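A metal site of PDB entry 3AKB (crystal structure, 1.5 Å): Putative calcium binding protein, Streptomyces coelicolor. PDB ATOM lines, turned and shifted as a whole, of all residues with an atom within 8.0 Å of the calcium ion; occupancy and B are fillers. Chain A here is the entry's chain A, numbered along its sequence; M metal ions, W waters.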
ATOM      1  N   HIS A  20      17.923  15.722 -27.471  1.00  0.00           N
ATOM      2  CA  HIS A  20      17.317  15.426 -26.197  1.00  0.00           C
ATOM      3  C   HIS A  20      18.155  14.363 -25.513  1.00  0.00           C
ATOM      4  O   HIS A  20      18.811  13.573 -26.178  1.00  0.00           O
ATOM      5  CB  HIS A  20      15.847  14.979 -26.353  1.00  0.00           C
ATOM      6  CG  HIS A  20      15.654  13.688 -27.103  1.00  0.00           C
ATOM      7  ND1 HIS A  20      15.283  13.639 -28.426  1.00  0.00           N
ATOM      8  CD2 HIS A  20      15.717  12.405 -26.666  1.00  0.00           C
ATOM      9  CE1 HIS A  20      15.168  12.377 -28.802  1.00  0.00           C
ATOM     10  NE2 HIS A  20      15.402  11.603 -27.745  1.00  0.00           N
ATOM     11  N   ILE A  21      18.125  14.359 -24.189  1.00  0.00           N
ATOM     12  CA  ILE A  21      18.909  13.411 -23.389  1.00  0.00           C
ATOM     13  C   ILE A  21      18.000  12.230 -23.018  1.00  0.00           C
ATOM     14  O   ILE A  21      16.908  12.442 -22.472  1.00  0.00           O
ATOM     15  CB  ILE A  21      19.455  14.081 -22.127  1.00  0.00           C
ATOM     16  CG1 ILE A  21      20.288  15.312 -22.513  1.00  0.00           C
ATOM     17  CG2 ILE A  21      20.315  13.081 -21.341  1.00  0.00           C
ATOM     18  CD1 ILE A  21      20.449  16.350 -21.421  1.00  0.00           C
ATOM     19  N   TRP A  57      21.835   8.903 -15.056  1.00  0.00           N
ATOM     20  CA  TRP A  57      20.651   9.231 -15.824  1.00  0.00           C
ATOM     21  C   TRP A  57      19.459   9.504 -14.910  1.00  0.00           C
ATOM     22  O   TRP A  57      18.784  10.505 -15.094  1.00  0.00           O
ATOM     23  CB  TRP A  57      20.338   8.068 -16.798  1.00  0.00           C
ATOM     24  CG  TRP A  57      18.891   8.067 -17.198  1.00  0.00           C
ATOM     25  CD1 TRP A  57      17.948   7.124 -16.847  1.00  0.00           C
ATOM     26  CD2 TRP A  57      18.206   9.049 -17.995  1.00  0.00           C
ATOM     27  NE1 TRP A  57      16.725   7.453 -17.395  1.00  0.00           N
ATOM     28  CE2 TRP A  57      16.856   8.634 -18.094  1.00  0.00           C
ATOM     29  CE3 TRP A  57      18.603  10.247 -18.628  1.00  0.00           C
ATOM     30  CZ2 TRP A  57      15.896   9.367 -18.819  1.00  0.00           C
ATOM     31  CZ3 TRP A  57      17.635  10.974 -19.333  1.00  0.00           C
ATOM     32  CH2 TRP A  57      16.301  10.529 -19.424  1.00  0.00           C
ATOM     33  N   ALA A  61      17.438  12.954 -14.815  1.00  0.00           N
ATOM     34  CA  ALA A  61      16.011  12.904 -15.137  1.00  0.00           C
ATOM     35  C   ALA A  61      15.181  13.417 -13.954  1.00  0.00           C
ATOM     36  O   ALA A  61      14.200  14.150 -14.159  1.00  0.00           O
ATOM     37  CB  ALA A  61      15.598  11.479 -15.529  1.00  0.00           C
ATOM     38  N   ALA A  64      15.465  17.244 -14.155  1.00  0.00           N
ATOM     39  CA  ALA A  64      15.185  17.948 -15.422  1.00  0.00           C
ATOM     40  C   ALA A  64      13.984  17.459 -16.231  1.00  0.00           C
ATOM     41  O   ALA A  64      13.415  18.231 -17.019  1.00  0.00           O
ATOM     42  CB  ALA A  64      16.430  17.919 -16.307  1.00  0.00           C
ATOM     43  N   ASP A  65      13.601  16.193 -16.056  1.00  0.00           N
ATOM     44  CA  ASP A  65      12.536  15.613 -16.879  1.00  0.00           C
ATOM     45  C   ASP A  65      11.187  15.924 -16.251  1.00  0.00           C
ATOM     46  O   ASP A  65      10.582  15.074 -15.608  1.00  0.00           O
ATOM     47  CB  ASP A  65      12.712  14.092 -17.035  1.00  0.00           C
ATOM     48  CG  ASP A  65      11.634  13.470 -17.890  1.00  0.00           C
ATOM     49  OD1 ASP A  65      11.061  14.162 -18.743  1.00  0.00           O
ATOM     50  OD2 ASP A  65      11.357  12.264 -17.726  1.00  0.00           O
ATOM     51  N   ARG A  66      10.698  17.133 -16.484  1.00  0.00           N
ATOM     52  CA  ARG A  66       9.527  17.606 -15.748  1.00  0.00           C
ATOM     53  C   ARG A  66       8.166  17.111 -16.269  1.00  0.00           C
ATOM     54  O   ARG A  66       7.178  17.140 -15.530  1.00  0.00           O
ATOM     55  CB  ARG A  66       9.576  19.120 -15.508  1.00  0.00           C
ATOM     56  CG  ARG A  66      10.587  19.549 -14.403  1.00  0.00           C
ATOM     57  CD  ARG A  66      10.280  18.884 -13.044  1.00  0.00           C
ATOM     58  NE  ARG A  66      11.485  18.704 -12.210  1.00  0.00           N
ATOM     59  CZ  ARG A  66      11.658  19.246 -11.010  1.00  0.00           C
ATOM     60  NH1 ARG A  66      10.696  19.993 -10.454  1.00  0.00           N
ATOM     61  NH2 ARG A  66      12.781  19.029 -10.339  1.00  0.00           N
ATOM     62  N   ASP A  67       8.125  16.598 -17.498  1.00  0.00           N
ATOM     63  CA  ASP A  67       6.895  16.012 -18.048  1.00  0.00           C
ATOM     64  C   ASP A  67       6.886  14.471 -18.030  1.00  0.00           C
ATOM     65  O   ASP A  67       5.929  13.851 -18.517  1.00  0.00           O
ATOM     66  CB  ASP A  67       6.561  16.590 -19.433  1.00  0.00           C
ATOM     67  CG  ASP A  67       7.552  16.192 -20.503  1.00  0.00           C
ATOM     68  OD1 ASP A  67       8.533  15.497 -20.172  1.00  0.00           O
ATOM     69  OD2 ASP A  67       7.359  16.569 -21.680  1.00  0.00           O
ATOM     70  N   GLY A  68       7.942  13.888 -17.468  1.00  0.00           N
ATOM     71  CA  GLY A  68       7.964  12.450 -17.158  1.00  0.00           C
ATOM     72  C   GLY A  68       8.094  11.480 -18.328  1.00  0.00           C
ATOM     73  O   GLY A  68       7.965  10.268 -18.132  1.00  0.00           O
ATOM     74  N   ASP A  69       8.367  11.989 -19.517  1.00  0.00           N
ATOM     75  CA  ASP A  69       8.421  11.154 -20.708  1.00  0.00           C
ATOM     76  C   ASP A  69       9.793  10.509 -20.901  1.00  0.00           C
ATOM     77  O   ASP A  69      10.011   9.840 -21.913  1.00  0.00           O
ATOM     78  CB  ASP A  69       7.982  11.931 -21.961  1.00  0.00           C
ATOM     79  CG  ASP A  69       8.981  12.995 -22.404  1.00  0.00           C
ATOM     80  OD1 ASP A  69       9.906  13.368 -21.628  1.00  0.00           O
ATOM     81  OD2 ASP A  69       8.835  13.467 -23.570  1.00  0.00           O
ATOM     82  N   GLN A  70      10.710  10.709 -19.945  1.00  0.00           N
ATOM     83  CA  GLN A  70      12.033  10.051 -19.981  1.00  0.00           C
ATOM     84  C   GLN A  70      12.882  10.445 -21.195  1.00  0.00           C
ATOM     85  O   GLN A  70      13.691   9.664 -21.721  1.00  0.00           O
ATOM     86  CB  GLN A  70      11.856   8.524 -19.792  1.00  0.00           C
ATOM     87  CG  GLN A  70      11.279   8.199 -18.400  1.00  0.00           C
ATOM     88  CD  GLN A  70      10.837   6.747 -18.229  1.00  0.00           C
ATOM     89  OE1 GLN A  70      10.848   5.958 -19.174  1.00  0.00           O
ATOM     90  NE2 GLN A  70      10.439   6.408 -17.005  1.00  0.00           N
ATOM     91  N   ARG A  71      12.652  11.674 -21.659  1.00  0.00           N
ATOM     92  CA  ARG A  71      13.503  12.415 -22.590  1.00  0.00           C
ATOM     93  C   ARG A  71      13.679  13.784 -21.919  1.00  0.00           C
ATOM     94  O   ARG A  71      12.704  14.368 -21.396  1.00  0.00           O
ATOM     95  CB  ARG A  71      12.838  12.614 -23.952  1.00  0.00           C
ATOM     96  CG  ARG A  71      12.631  11.345 -24.776  1.00  0.00           C
ATOM     97  CD  ARG A  71      12.030  11.666 -26.137  1.00  0.00           C
ATOM     98  NE  ARG A  71      10.641  12.042 -25.965  1.00  0.00           N
ATOM     99  CZ  ARG A  71       9.623  11.195 -26.113  1.00  0.00           C
ATOM    100  NH1 ARG A  71       9.883   9.939 -26.459  1.00  0.00           N
ATOM    101  NH2 ARG A  71       8.386  11.613 -25.934  1.00  0.00           N
ATOM    102  N   ILE A  72      14.903  14.288 -21.893  1.00  0.00           N
ATOM    103  CA  ILE A  72      15.133  15.648 -21.398  1.00  0.00           C
ATOM    104  C   ILE A  72      15.432  16.523 -22.599  1.00  0.00           C
ATOM    105  O   ILE A  72      16.469  16.378 -23.237  1.00  0.00           O
ATOM    106  CB  ILE A  72      16.346  15.712 -20.439  1.00  0.00           C
ATOM    107  CG1 ILE A  72      16.129  14.757 -19.249  1.00  0.00           C
ATOM    108  CG2 ILE A  72      16.570  17.157 -19.966  1.00  0.00           C
ATOM    109  CD1 ILE A  72      17.407  14.478 -18.435  1.00  0.00           C
ATOM    110  N   THR A  73      14.500  17.426 -22.923  1.00  0.00           N
ATOM    111  CA  THR A  73      14.688  18.328 -24.046  1.00  0.00           C
ATOM    112  C   THR A  73      15.684  19.445 -23.716  1.00  0.00           C
ATOM    113  O   THR A  73      15.957  19.706 -22.539  1.00  0.00           O
ATOM    114  CB  THR A  73      13.354  18.963 -24.479  1.00  0.00           C
ATOM    115  OG1 THR A  73      12.803  19.702 -23.388  1.00  0.00           O
ATOM    116  CG2 THR A  73      12.361  17.914 -24.916  1.00  0.00           C
ATOM    117  N   GLU A  76      13.842  21.802 -21.427  1.00  0.00           N
ATOM    118  CA  GLU A  76      13.824  21.301 -20.055  1.00  0.00           C
ATOM    119  C   GLU A  76      15.162  21.525 -19.338  1.00  0.00           C
ATOM    120  O   GLU A  76      15.209  21.852 -18.142  1.00  0.00           O
ATOM    121  CB  GLU A  76      13.470  19.808 -20.045  1.00  0.00           C
ATOM    122  CG  GLU A  76      11.976  19.562 -20.176  1.00  0.00           C
ATOM    123  CD  GLU A  76      11.622  18.075 -20.250  1.00  0.00           C
ATOM    124  OE1 GLU A  76      12.343  17.321 -20.908  1.00  0.00           O
ATOM    125  OE2 GLU A  76      10.620  17.662 -19.641  1.00  0.00           O
HETATM  126 CA    CA M   1      10.759  15.384 -20.808  1.00  0.00          CA
HETATM  127  O   HOH W   1       9.987  16.200 -23.059  1.00  0.00           O
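N of Arg 66 lies close to OE2 of Glu 76. OD2 of Asp 65 lies within hydrogen-bond range of N of Gln 70. The backbone NH (N) of Glu 76 lies within hydrogen-bond range of the side-chain hydroxyl (OG1) of Thr 73, 3.1 Å away. OD1 of Asp 65 sits close to N of Gly 68, 3.4 Å away.
Water W1 bridges the side-chain carboxylate (OD2) of Asp 67 (3.0 Å) and the side-chain carboxylate (OD2) of Asp 69 (3.0 Å).
Of the 15 residues printed, 5 come within 4 Å of the calcium ion. The nearest printed residue that does not touch the calcium ion is Ile 72 (4.4 Å).
The calcium ion is bound by O of Arg 71 (2.3 Å). The calcium ion is bound by OD1 of Asp 67 (2.3 Å). OD1 of Asp 69 binds the calcium ion. The calcium ion is bound by OD1 of Asp 65 (2.4 Å). OE1 of Glu 76 is bound to the calcium ion (2.5 Å). Water W1 is bound to the calcium ion. The side-chain carboxylate (OE2) of Glu 76 binds the calcium ion, at 2.6 Å.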
